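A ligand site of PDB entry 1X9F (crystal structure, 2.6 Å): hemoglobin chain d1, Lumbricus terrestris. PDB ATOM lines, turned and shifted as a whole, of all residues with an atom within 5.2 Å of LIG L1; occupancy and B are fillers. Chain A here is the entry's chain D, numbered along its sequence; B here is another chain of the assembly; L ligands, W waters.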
ATOM      1  N   TRP A  32      20.334   0.630   6.332  1.00  0.00           N
ATOM      2  CA  TRP A  32      21.128   1.594   5.549  1.00  0.00           C
ATOM      3  C   TRP A  32      21.365   2.914   6.237  1.00  0.00           C
ATOM      4  O   TRP A  32      22.395   3.537   6.022  1.00  0.00           O
ATOM      5  CB  TRP A  32      20.533   1.831   4.154  1.00  0.00           C
ATOM      6  CG  TRP A  32      20.798   0.661   3.336  1.00  0.00           C
ATOM      7  CD1 TRP A  32      19.903  -0.288   2.980  1.00  0.00           C
ATOM      8  CD2 TRP A  32      22.067   0.258   2.820  1.00  0.00           C
ATOM      9  NE1 TRP A  32      20.536  -1.272   2.245  1.00  0.00           N
ATOM     10  CE2 TRP A  32      21.860  -0.952   2.129  1.00  0.00           C
ATOM     11  CE3 TRP A  32      23.357   0.797   2.856  1.00  0.00           C
ATOM     12  CZ2 TRP A  32      22.892  -1.627   1.490  1.00  0.00           C
ATOM     13  CZ3 TRP A  32      24.384   0.131   2.216  1.00  0.00           C
ATOM     14  CH2 TRP A  32      24.145  -1.071   1.542  1.00  0.00           C
ATOM     15  N   ILE A  42      29.772   6.010   1.771  1.00  0.00           N
ATOM     16  CA  ILE A  42      28.948   4.987   1.124  1.00  0.00           C
ATOM     17  C   ILE A  42      27.785   5.550   0.293  1.00  0.00           C
ATOM     18  O   ILE A  42      27.201   4.827  -0.516  1.00  0.00           O
ATOM     19  CB  ILE A  42      28.480   3.915   2.149  1.00  0.00           C
ATOM     20  CG1 ILE A  42      29.690   3.133   2.671  1.00  0.00           C
ATOM     21  CG2 ILE A  42      27.485   2.953   1.529  1.00  0.00           C
ATOM     22  CD1 ILE A  42      29.410   2.232   3.867  1.00  0.00           C
ATOM     23  N   PRO A  45      28.574   5.829  -4.111  1.00  0.00           N
ATOM     24  CA  PRO A  45      28.185   4.802  -5.067  1.00  0.00           C
ATOM     25  C   PRO A  45      26.679   4.622  -5.211  1.00  0.00           C
ATOM     26  O   PRO A  45      26.237   4.006  -6.175  1.00  0.00           O
ATOM     27  CB  PRO A  45      28.834   3.532  -4.499  1.00  0.00           C
ATOM     28  CG  PRO A  45      28.943   3.787  -3.062  1.00  0.00           C
ATOM     29  CD  PRO A  45      29.246   5.244  -2.934  1.00  0.00           C
ATOM     30  N   PHE A  46      25.885   5.172  -4.278  1.00  0.00           N
ATOM     31  CA  PHE A  46      24.410   5.060  -4.334  1.00  0.00           C
ATOM     32  C   PHE A  46      23.763   6.248  -5.038  1.00  0.00           C
ATOM     33  O   PHE A  46      22.583   6.557  -4.843  1.00  0.00           O
ATOM     34  CB  PHE A  46      23.836   4.906  -2.932  1.00  0.00           C
ATOM     35  CG  PHE A  46      24.132   3.577  -2.309  1.00  0.00           C
ATOM     36  CD1 PHE A  46      24.450   3.479  -0.961  1.00  0.00           C
ATOM     37  CD2 PHE A  46      24.128   2.419  -3.077  1.00  0.00           C
ATOM     38  CE1 PHE A  46      24.729   2.258  -0.394  1.00  0.00           C
ATOM     39  CE2 PHE A  46      24.414   1.199  -2.522  1.00  0.00           C
ATOM     40  CZ  PHE A  46      24.714   1.114  -1.174  1.00  0.00           C
ATOM     41  N   ARG A  48      22.935   6.772  -8.189  1.00  0.00           N
ATOM     42  CA  ARG A  48      21.859   6.448  -9.119  1.00  0.00           C
ATOM     43  C   ARG A  48      20.558   6.057  -8.414  1.00  0.00           C
ATOM     44  O   ARG A  48      19.491   6.042  -9.027  1.00  0.00           O
ATOM     45  CB  ARG A  48      22.331   5.313 -10.052  1.00  0.00           C
ATOM     46  CG  ARG A  48      21.725   5.310 -11.458  1.00  0.00           C
ATOM     47  CD  ARG A  48      20.436   4.470 -11.619  1.00  0.00           C
ATOM     48  NE  ARG A  48      20.643   3.048 -11.345  1.00  0.00           N
ATOM     49  CZ  ARG A  48      19.666   2.151 -11.192  1.00  0.00           C
ATOM     50  NH1 ARG A  48      18.386   2.515 -11.272  1.00  0.00           N
ATOM     51  NH2 ARG A  48      19.966   0.879 -10.952  1.00  0.00           N
ATOM     52  N   VAL A  49      20.629   5.755  -7.111  1.00  0.00           N
ATOM     53  CA  VAL A  49      19.453   5.298  -6.385  1.00  0.00           C
ATOM     54  C   VAL A  49      19.023   6.220  -5.236  1.00  0.00           C
ATOM     55  O   VAL A  49      18.355   5.773  -4.297  1.00  0.00           O
ATOM     56  CB  VAL A  49      19.623   3.834  -5.866  1.00  0.00           C
ATOM     57  CG1 VAL A  49      19.749   2.857  -7.030  1.00  0.00           C
ATOM     58  CG2 VAL A  49      20.819   3.718  -4.915  1.00  0.00           C
ATOM     59  N   HIS A  62      15.945   0.091  -4.133  1.00  0.00           N
ATOM     60  CA  HIS A  62      17.293  -0.459  -4.017  1.00  0.00           C
ATOM     61  C   HIS A  62      17.452  -1.273  -2.735  1.00  0.00           C
ATOM     62  O   HIS A  62      17.904  -2.421  -2.769  1.00  0.00           O
ATOM     63  CB  HIS A  62      18.361   0.655  -4.086  1.00  0.00           C
ATOM     64  CG  HIS A  62      19.722   0.187  -3.696  1.00  0.00           C
ATOM     65  ND1 HIS A  62      20.484  -0.613  -4.510  1.00  0.00           N
ATOM     66  CD2 HIS A  62      20.430   0.368  -2.567  1.00  0.00           C
ATOM     67  CE1 HIS A  62      21.627  -0.894  -3.904  1.00  0.00           C
ATOM     68  NE2 HIS A  62      21.621  -0.311  -2.724  1.00  0.00           N
ATOM     69  N   ARG A  65      15.782  -4.543  -3.024  1.00  0.00           N
ATOM     70  CA  ARG A  65      16.564  -5.395  -3.925  1.00  0.00           C
ATOM     71  C   ARG A  65      17.727  -6.044  -3.183  1.00  0.00           C
ATOM     72  O   ARG A  65      18.059  -7.210  -3.451  1.00  0.00           O
ATOM     73  CB  ARG A  65      17.073  -4.628  -5.150  1.00  0.00           C
ATOM     74  CG  ARG A  65      15.984  -4.364  -6.183  1.00  0.00           C
ATOM     75  CD  ARG A  65      16.505  -3.943  -7.554  1.00  0.00           C
ATOM     76  NE  ARG A  65      17.123  -2.612  -7.549  1.00  0.00           N
ATOM     77  CZ  ARG A  65      16.457  -1.464  -7.619  1.00  0.00           C
ATOM     78  NH1 ARG A  65      15.127  -1.440  -7.687  1.00  0.00           N
ATOM     79  NH2 ARG A  65      17.125  -0.323  -7.594  1.00  0.00           N
ATOM     80  N   VAL A  66      18.335  -5.308  -2.254  1.00  0.00           N
ATOM     81  CA  VAL A  66      19.448  -5.824  -1.458  1.00  0.00           C
ATOM     82  C   VAL A  66      18.997  -6.924  -0.505  1.00  0.00           C
ATOM     83  O   VAL A  66      19.613  -7.989  -0.461  1.00  0.00           O
ATOM     84  CB  VAL A  66      20.094  -4.724  -0.622  1.00  0.00           C
ATOM     85  CG1 VAL A  66      21.223  -5.297   0.255  1.00  0.00           C
ATOM     86  CG2 VAL A  66      20.581  -3.630  -1.528  1.00  0.00           C
ATOM     87  N   GLY A  69      18.188  -9.973  -2.202  1.00  0.00           N
ATOM     88  CA  GLY A  69      19.454 -10.596  -2.586  1.00  0.00           C
ATOM     89  C   GLY A  69      20.054 -11.403  -1.454  1.00  0.00           C
ATOM     90  O   GLY A  69      20.465 -12.555  -1.639  1.00  0.00           O
ATOM     91  N   LEU A  70      20.085 -10.786  -0.264  1.00  0.00           N
ATOM     92  CA  LEU A  70      20.558 -11.466   0.926  1.00  0.00           C
ATOM     93  C   LEU A  70      19.711 -12.693   1.158  1.00  0.00           C
ATOM     94  O   LEU A  70      20.210 -13.746   1.539  1.00  0.00           O
ATOM     95  CB  LEU A  70      20.446 -10.531   2.134  1.00  0.00           C
ATOM     96  CG  LEU A  70      21.644 -10.404   3.075  1.00  0.00           C
ATOM     97  CD1 LEU A  70      21.194  -9.649   4.322  1.00  0.00           C
ATOM     98  CD2 LEU A  70      22.243 -11.750   3.453  1.00  0.00           C
ATOM     99  N   LEU A  90      26.335 -11.825  -8.065  1.00  0.00           N
ATOM    100  CA  LEU A  90      26.261 -10.629  -7.245  1.00  0.00           C
ATOM    101  C   LEU A  90      27.549  -9.841  -7.350  1.00  0.00           C
ATOM    102  O   LEU A  90      27.537  -8.603  -7.330  1.00  0.00           O
ATOM    103  CB  LEU A  90      25.976 -10.997  -5.795  1.00  0.00           C
ATOM    104  CG  LEU A  90      24.485 -11.091  -5.469  1.00  0.00           C
ATOM    105  CD1 LEU A  90      24.284 -11.887  -4.200  1.00  0.00           C
ATOM    106  CD2 LEU A  90      23.876  -9.700  -5.344  1.00  0.00           C
ATOM    107  N   GLN A  93      27.754  -7.702 -10.340  1.00  0.00           N
ATOM    108  CA  GLN A  93      26.897  -6.544 -10.107  1.00  0.00           C
ATOM    109  C   GLN A  93      27.520  -5.509  -9.177  1.00  0.00           C
ATOM    110  O   GLN A  93      26.993  -4.407  -9.040  1.00  0.00           O
ATOM    111  CB  GLN A  93      25.556  -6.992  -9.524  1.00  0.00           C
ATOM    112  CG  GLN A  93      24.658  -7.682 -10.519  1.00  0.00           C
ATOM    113  CD  GLN A  93      23.389  -8.157  -9.860  1.00  0.00           C
ATOM    114  OE1 GLN A  93      23.402  -8.564  -8.690  1.00  0.00           O
ATOM    115  NE2 GLN A  93      22.286  -8.111 -10.593  1.00  0.00           N
ATOM    116  N   HIS A  94      28.627  -5.863  -8.545  1.00  0.00           N
ATOM    117  CA  HIS A  94      29.293  -4.926  -7.648  1.00  0.00           C
ATOM    118  C   HIS A  94      30.698  -4.515  -8.126  1.00  0.00           C
ATOM    119  O   HIS A  94      31.211  -3.476  -7.703  1.00  0.00           O
ATOM    120  CB  HIS A  94      29.347  -5.504  -6.221  1.00  0.00           C
ATOM    121  CG  HIS A  94      27.996  -5.548  -5.557  1.00  0.00           C
ATOM    122  ND1 HIS A  94      27.067  -6.522  -5.829  1.00  0.00           N
ATOM    123  CD2 HIS A  94      27.438  -4.740  -4.628  1.00  0.00           C
ATOM    124  CE1 HIS A  94      25.984  -6.312  -5.101  1.00  0.00           C
ATOM    125  NE2 HIS A  94      26.190  -5.232  -4.364  1.00  0.00           N
ATOM    126  N   ARG A  97      32.218  -0.835  -9.551  1.00  0.00           N
ATOM    127  CA  ARG A  97      31.955   0.363  -8.777  1.00  0.00           C
ATOM    128  C   ARG A  97      33.092   0.474  -7.801  1.00  0.00           C
ATOM    129  O   ARG A  97      33.639  -0.554  -7.366  1.00  0.00           O
ATOM    130  CB  ARG A  97      30.603   0.218  -8.089  1.00  0.00           C
ATOM    131  CG  ARG A  97      29.540  -0.304  -9.062  1.00  0.00           C
ATOM    132  CD  ARG A  97      28.307  -0.887  -8.408  1.00  0.00           C
ATOM    133  NE  ARG A  97      27.329  -1.340  -9.386  1.00  0.00           N
ATOM    134  CZ  ARG A  97      26.555  -0.541 -10.115  1.00  0.00           C
ATOM    135  NH1 ARG A  97      26.635   0.781  -9.987  1.00  0.00           N
ATOM    136  NH2 ARG A  97      25.682  -1.052 -10.971  1.00  0.00           N
ATOM    137  N   LEU A  99      33.893   0.253  -4.923  1.00  0.00           N
ATOM    138  CA  LEU A  99      33.534  -0.202  -3.597  1.00  0.00           C
ATOM    139  C   LEU A  99      34.766  -0.756  -2.920  1.00  0.00           C
ATOM    140  O   LEU A  99      35.401  -1.685  -3.434  1.00  0.00           O
ATOM    141  CB  LEU A  99      32.429  -1.264  -3.635  1.00  0.00           C
ATOM    142  CG  LEU A  99      31.185  -1.058  -4.516  1.00  0.00           C
ATOM    143  CD1 LEU A  99      30.148  -2.123  -4.221  1.00  0.00           C
ATOM    144  CD2 LEU A  99      30.594   0.340  -4.344  1.00  0.00           C
ATOM    145  N   PHE A 103      33.666  -1.922   2.837  1.00  0.00           N
ATOM    146  CA  PHE A 103      32.253  -1.567   2.797  1.00  0.00           C
ATOM    147  C   PHE A 103      31.377  -2.741   3.205  1.00  0.00           C
ATOM    148  O   PHE A 103      30.451  -2.591   4.008  1.00  0.00           O
ATOM    149  CB  PHE A 103      31.850  -1.071   1.410  1.00  0.00           C
ATOM    150  CG  PHE A 103      32.317   0.315   1.110  1.00  0.00           C
ATOM    151  CD1 PHE A 103      32.160   0.853  -0.164  1.00  0.00           C
ATOM    152  CD2 PHE A 103      32.918   1.092   2.093  1.00  0.00           C
ATOM    153  CE1 PHE A 103      32.572   2.141  -0.447  1.00  0.00           C
ATOM    154  CE2 PHE A 103      33.351   2.371   1.818  1.00  0.00           C
ATOM    155  CZ  PHE A 103      33.172   2.910   0.550  1.00  0.00           C
ATOM    156  N   PHE A 104      31.678  -3.910   2.651  1.00  0.00           N
ATOM    157  CA  PHE A 104      30.936  -5.133   2.961  1.00  0.00           C
ATOM    158  C   PHE A 104      31.142  -5.528   4.413  1.00  0.00           C
ATOM    159  O   PHE A 104      30.209  -6.029   5.051  1.00  0.00           O
ATOM    160  CB  PHE A 104      31.332  -6.257   2.002  1.00  0.00           C
ATOM    161  CG  PHE A 104      30.986  -5.945   0.576  1.00  0.00           C
ATOM    162  CD1 PHE A 104      31.833  -5.143  -0.176  1.00  0.00           C
ATOM    163  CD2 PHE A 104      29.803  -6.397   0.018  1.00  0.00           C
ATOM    164  CE1 PHE A 104      31.518  -4.818  -1.495  1.00  0.00           C
ATOM    165  CE2 PHE A 104      29.478  -6.076  -1.296  1.00  0.00           C
ATOM    166  CZ  PHE A 104      30.333  -5.294  -2.055  1.00  0.00           C
ATOM    167  N   PHE A 107      28.947  -3.369   6.245  1.00  0.00           N
ATOM    168  CA  PHE A 107      27.608  -3.877   6.025  1.00  0.00           C
ATOM    169  C   PHE A 107      27.279  -4.996   7.016  1.00  0.00           C
ATOM    170  O   PHE A 107      26.254  -4.945   7.707  1.00  0.00           O
ATOM    171  CB  PHE A 107      27.449  -4.389   4.604  1.00  0.00           C
ATOM    172  CG  PHE A 107      26.102  -4.973   4.315  1.00  0.00           C
ATOM    173  CD1 PHE A 107      25.113  -4.213   3.705  1.00  0.00           C
ATOM    174  CD2 PHE A 107      25.817  -6.295   4.661  1.00  0.00           C
ATOM    175  CE1 PHE A 107      23.854  -4.755   3.441  1.00  0.00           C
ATOM    176  CE2 PHE A 107      24.563  -6.845   4.399  1.00  0.00           C
ATOM    177  CZ  PHE A 107      23.591  -6.077   3.782  1.00  0.00           C
ATOM    178  N   ILE A 135      29.246 -15.357   2.579  1.00  0.00           N
ATOM    179  CA  ILE A 135      28.486 -14.641   1.558  1.00  0.00           C
ATOM    180  C   ILE A 135      29.177 -13.335   1.222  1.00  0.00           C
ATOM    181  O   ILE A 135      29.422 -13.054   0.044  1.00  0.00           O
ATOM    182  CB  ILE A 135      27.020 -14.382   2.016  1.00  0.00           C
ATOM    183  CG1 ILE A 135      26.264 -15.701   2.167  1.00  0.00           C
ATOM    184  CG2 ILE A 135      26.296 -13.484   0.997  1.00  0.00           C
ATOM    185  CD1 ILE A 135      24.954 -15.551   2.937  1.00  0.00           C
ATOM    186  N   ILE A 136      29.495 -12.535   2.234  1.00  0.00           N
ATOM    187  CA  ILE A 136      30.239 -11.304   2.019  1.00  0.00           C
ATOM    188  C   ILE A 136      31.532 -11.538   1.227  1.00  0.00           C
ATOM    189  O   ILE A 136      31.817 -10.767   0.306  1.00  0.00           O
ATOM    190  CB  ILE A 136      30.502 -10.575   3.367  1.00  0.00           C
ATOM    191  CG1 ILE A 136      29.542  -9.396   3.524  1.00  0.00           C
ATOM    192  CG2 ILE A 136      31.912 -10.018   3.451  1.00  0.00           C
ATOM    193  CD1 ILE A 136      28.166  -9.788   3.954  1.00  0.00           C
ATOM    194  N   ILE A 139      31.272 -11.817  -2.616  1.00  0.00           N
ATOM    195  CA  ILE A 139      30.856 -10.623  -3.355  1.00  0.00           C
ATOM    196  C   ILE A 139      31.935  -9.567  -3.275  1.00  0.00           C
ATOM    197  O   ILE A 139      32.171  -8.832  -4.236  1.00  0.00           O
ATOM    198  CB  ILE A 139      29.527 -10.079  -2.772  1.00  0.00           C
ATOM    199  CG1 ILE A 139      28.462 -11.180  -2.763  1.00  0.00           C
ATOM    200  CG2 ILE A 139      29.053  -8.872  -3.575  1.00  0.00           C
ATOM    201  CD1 ILE A 139      27.234 -10.867  -1.931  1.00  0.00           C
ATOM    202  N   HIS B  96      12.961  -0.591 -12.710  1.00  0.00           N
ATOM    203  CA  HIS B  96      14.246  -1.273 -12.607  1.00  0.00           C
ATOM    204  C   HIS B  96      14.183  -2.651 -13.259  1.00  0.00           C
ATOM    205  O   HIS B  96      15.059  -3.003 -14.065  1.00  0.00           O
ATOM    206  CB  HIS B  96      14.674  -1.391 -11.141  1.00  0.00           C
ATOM    207  CG  HIS B  96      16.023  -2.034 -10.960  1.00  0.00           C
ATOM    208  ND1 HIS B  96      17.175  -1.301 -10.842  1.00  0.00           N
ATOM    209  CD2 HIS B  96      16.380  -3.329 -10.882  1.00  0.00           C
ATOM    210  CE1 HIS B  96      18.203  -2.128 -10.692  1.00  0.00           C
ATOM    211  NE2 HIS B  96      17.739  -3.363 -10.708  1.00  0.00           N
ATOM    212  N   GLN B 100      16.164  -4.140 -16.724  1.00  0.00           N
ATOM    213  CA  GLN B 100      16.927  -5.386 -16.780  1.00  0.00           C
ATOM    214  C   GLN B 100      16.512  -6.251 -17.971  1.00  0.00           C
ATOM    215  O   GLN B 100      17.352  -6.921 -18.579  1.00  0.00           O
ATOM    216  CB  GLN B 100      16.796  -6.157 -15.463  1.00  0.00           C
ATOM    217  CG  GLN B 100      17.576  -5.527 -14.315  1.00  0.00           C
ATOM    218  CD  GLN B 100      17.474  -6.310 -13.024  1.00  0.00           C
ATOM    219  OE1 GLN B 100      16.378  -6.686 -12.592  1.00  0.00           O
ATOM    220  NE2 GLN B 100      18.611  -6.540 -12.379  1.00  0.00           N
HETATM  221  C1  LIG L   1      23.225  -3.171  -6.073  1.00  0.00           C
HETATM  222  C2  LIG L   1      23.048  -7.088  -3.181  1.00  0.00           C
HETATM  223  C3  LIG L   1      26.264  -5.038  -0.119  1.00  0.00           C
HETATM  224  C4  LIG L   1      26.697  -1.256  -3.245  1.00  0.00           C
HETATM  225  C5  LIG L   1      22.817  -4.442  -5.468  1.00  0.00           C
HETATM  226  C6  LIG L   1      21.832  -5.188  -6.079  1.00  0.00           C
HETATM  227  C7  LIG L   1      21.728  -6.387  -5.256  1.00  0.00           C
HETATM  228  C8  LIG L   1      22.752  -6.121  -4.236  1.00  0.00           C
HETATM  229  C9  LIG L   1      20.808  -7.571  -5.435  1.00  0.00           C
HETATM  230  C10 LIG L   1      21.024  -4.802  -7.289  1.00  0.00           C
HETATM  231  C11 LIG L   1      21.470  -5.463  -8.578  1.00  0.00           C
HETATM  232  C12 LIG L   1      20.443  -5.011  -9.596  1.00  0.00           C
HETATM  233  O1  LIG L   1      19.276  -5.462  -9.534  1.00  0.00           O
HETATM  234  O2  LIG L   1      20.807  -4.196 -10.457  1.00  0.00           O
HETATM  235  C13 LIG L   1      23.966  -6.864  -2.073  1.00  0.00           C
HETATM  236  C14 LIG L   1      24.067  -7.793  -1.041  1.00  0.00           C
HETATM  237  C15 LIG L   1      24.945  -7.161  -0.229  1.00  0.00           C
HETATM  238  C16 LIG L   1      25.338  -5.965  -0.760  1.00  0.00           C
HETATM  239  C17 LIG L   1      23.384  -9.136  -0.859  1.00  0.00           C
HETATM  240  C18 LIG L   1      25.351  -7.741   0.890  1.00  0.00           C
HETATM  241  C19 LIG L   1      25.832  -8.510   1.900  1.00  0.00           C
HETATM  242  C20 LIG L   1      26.651  -3.742  -0.716  1.00  0.00           C
HETATM  243  C21 LIG L   1      27.528  -2.896  -0.055  1.00  0.00           C
HETATM  244  C22 LIG L   1      27.649  -1.861  -0.935  1.00  0.00           C
HETATM  245  C23 LIG L   1      26.827  -2.099  -2.033  1.00  0.00           C
HETATM  246  C24 LIG L   1      28.225  -3.076   1.280  1.00  0.00           C
HETATM  247  C25 LIG L   1      28.508  -0.697  -0.567  1.00  0.00           C
HETATM  248  C26 LIG L   1      28.927   0.269  -1.518  1.00  0.00           C
HETATM  249  C27 LIG L   1      25.773  -1.465  -4.379  1.00  0.00           C
HETATM  250  C28 LIG L   1      25.621  -0.529  -5.410  1.00  0.00           C
HETATM  251  C29 LIG L   1      24.637  -1.048  -6.232  1.00  0.00           C
HETATM  252  C30 LIG L   1      24.287  -2.310  -5.569  1.00  0.00           C
HETATM  253  C31 LIG L   1      26.376   0.761  -5.594  1.00  0.00           C
HETATM  254  C32 LIG L   1      24.066  -0.497  -7.512  1.00  0.00           C
HETATM  255  C33 LIG L   1      22.924   0.470  -7.263  1.00  0.00           C
HETATM  256  C34 LIG L   1      22.436   0.888  -8.631  1.00  0.00           C
HETATM  257  O3  LIG L   1      21.870   0.029  -9.354  1.00  0.00           O
HETATM  258  O4  LIG L   1      22.616   2.068  -8.986  1.00  0.00           O
HETATM  259  N1  LIG L   1      23.431  -4.958  -4.376  1.00  0.00           N
HETATM  260  N2  LIG L   1      24.715  -5.737  -1.935  1.00  0.00           N
HETATM  261  N3  LIG L   1      26.224  -3.308  -1.931  1.00  0.00           N
HETATM  262  N4  LIG L   1      24.970  -2.547  -4.430  1.00  0.00           N
HETATM  263 FE1  LIG L   1      24.861  -4.143  -3.182  1.00  0.00          FE
HETATM  264  C1  LG2 L   2      23.390  -3.065  -1.824  1.00  0.00           C
HETATM  265  O1  LG2 L   2      23.415  -1.781  -1.436  1.00  0.00           O
HETATM  266  C1  LG3 L   3      16.738 -12.343 -15.793  1.00  0.00           C
HETATM  267  C2  LG3 L   3      12.839 -11.559 -12.927  1.00  0.00           C
HETATM  268  C3  LG3 L   3       9.900 -12.649 -16.679  1.00  0.00           C
HETATM  269  C4  LG3 L   3      13.785 -13.224 -19.624  1.00  0.00           C
HETATM  270  C5  LG3 L   3      15.896 -12.040 -14.617  1.00  0.00           C
HETATM  271  C6  LG3 L   3      16.449 -11.704 -13.378  1.00  0.00           C
HETATM  272  C7  LG3 L   3      15.306 -11.474 -12.497  1.00  0.00           C
HETATM  273  C8  LG3 L   3      14.200 -11.710 -13.426  1.00  0.00           C
HETATM  274  C9  LG3 L   3      15.260 -11.069 -11.035  1.00  0.00           C
HETATM  275  C10 LG3 L   3      17.894 -11.609 -12.956  1.00  0.00           C
HETATM  276  C11 LG3 L   3      18.375 -10.177 -13.177  1.00  0.00           C
HETATM  277  C12 LG3 L   3      19.822 -10.191 -12.784  1.00  0.00           C
HETATM  278  O1  LG3 L   3      20.113 -10.087 -11.576  1.00  0.00           O
HETATM  279  O2  LG3 L   3      20.683 -10.313 -13.677  1.00  0.00           O
HETATM  280  C13 LG3 L   3      11.645 -11.776 -13.740  1.00  0.00           C
HETATM  281  C14 LG3 L   3      10.380 -11.655 -13.192  1.00  0.00           C
HETATM  282  C15 LG3 L   3       9.640 -11.939 -14.286  1.00  0.00           C
HETATM  283  C16 LG3 L   3      10.425 -12.255 -15.364  1.00  0.00           C
HETATM  284  C17 LG3 L   3       9.916 -11.261 -11.793  1.00  0.00           C
HETATM  285  C18 LG3 L   3       8.306 -11.988 -14.306  1.00  0.00           C
HETATM  286  C19 LG3 L   3       6.950 -12.127 -14.178  1.00  0.00           C
HETATM  287  C20 LG3 L   3      10.731 -12.913 -17.865  1.00  0.00           C
HETATM  288  C21 LG3 L   3      10.183 -13.212 -19.107  1.00  0.00           C
HETATM  289  C22 LG3 L   3      11.298 -13.370 -19.896  1.00  0.00           C
HETATM  290  C23 LG3 L   3      12.407 -13.147 -19.105  1.00  0.00           C
HETATM  291  C24 LG3 L   3       8.730 -13.342 -19.504  1.00  0.00           C
HETATM  292  C25 LG3 L   3      11.300 -13.671 -21.349  1.00  0.00           C
HETATM  293  C26 LG3 L   3      11.362 -14.923 -21.828  1.00  0.00           C
HETATM  294  C27 LG3 L   3      15.007 -13.013 -18.806  1.00  0.00           C
HETATM  295  C28 LG3 L   3      16.281 -13.131 -19.359  1.00  0.00           C
HETATM  296  C29 LG3 L   3      17.143 -12.891 -18.305  1.00  0.00           C
HETATM  297  C30 LG3 L   3      16.250 -12.632 -17.154  1.00  0.00           C
HETATM  298  C31 LG3 L   3      16.646 -13.446 -20.789  1.00  0.00           C
HETATM  299  C32 LG3 L   3      18.642 -12.857 -18.305  1.00  0.00           C
HETATM  300  C33 LG3 L   3      19.183 -14.196 -17.837  1.00  0.00           C
HETATM  301  C34 LG3 L   3      20.687 -14.024 -17.733  1.00  0.00           C
HETATM  302  O3  LG3 L   3      21.376 -14.132 -18.780  1.00  0.00           O
HETATM  303  O4  LG3 L   3      21.164 -13.763 -16.611  1.00  0.00           O
HETATM  304  N1  LG3 L   3      14.540 -12.043 -14.691  1.00  0.00           N
HETATM  305  N2  LG3 L   3      11.723 -12.159 -15.055  1.00  0.00           N
HETATM  306  N3  LG3 L   3      12.091 -12.867 -17.819  1.00  0.00           N
HETATM  307  N4  LG3 L   3      14.936 -12.727 -17.471  1.00  0.00           N
HETATM  308 FE1  LG3 L   3      13.337 -12.479 -16.258  1.00  0.00          FE
HETATM  309  O   HOH W   1      23.588   4.057  -7.424  1.00  0.00           O
HETATM  310  O   HOH W   2      17.952  -7.247  -8.532  1.00  0.00           O
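A ring nitrogen (NE2) of His 94 is bound to an iron atom (FE1) of LIG L1 (2.1 Å). The guanidinium group of Arg 48 lies within salt-bridge range of an oxygen (O3) of LIG L1, 2.6 Å away. An oxygen (O1) of LIG L1 lies within hydrogen-bond range of a ring nitrogen (NE2) of His 96 of chain B, 2.9 Å away. The side-chain amide nitrogen (NE2) of Gln 100 of chain B lies within hydrogen-bond range of an oxygen (O1) of LIG L1, 3.1 Å away. O1 of LG2 L2 lies within hydrogen-bond range of NE2 of His 62. The side-chain amide nitrogen (NE2) of Gln 93 sits at hydrogen-bond distance from an oxygen (O1) of LG3 L3, 3.1 Å away.
A ring nitrogen (ND1) of His 94 sits at hydrogen-bond distance from the backbone carbonyl oxygen (O) of Leu 90, 2.6 Å away. NE of Arg 65 is in hydrogen-bond range of NE2 of His 96 of chain B (3.3 Å). The guanidinium group (NE) of Arg 97 is in hydrogen-bond range of the backbone carbonyl oxygen (O) of Gln 93.
Merely in contact with LIG L1: Pro 45, Phe 46, Val 49, His 62, Arg 65, Val 66, Leu 70, Leu 90, Gln 93, Arg 97, Leu 99, Phe 103, Phe 104, Phe 107 and Ile 136. Within 4 Å of LIG L1: Pro 45, Phe 46, Arg 48, Val 49, His 62, Arg 65, Val 66, Leu 70, Leu 90, Gln 93, His 94, Arg 97, Leu 99, Phe 103, Phe 104, Phe 107, Ile 136, His 96 of chain B and Gln 100 of chain B. The nearest printed residue that does not touch LIG L1 is Gly 69 (4.1 Å).
Water W1 lies within hydrogen-bond range of O4 of LIG L1 (2.7 Å), N of Arg 48 (2.9 Å), O of Pro 45 (2.9 Å) and N of Val 49 (3.4 Å).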
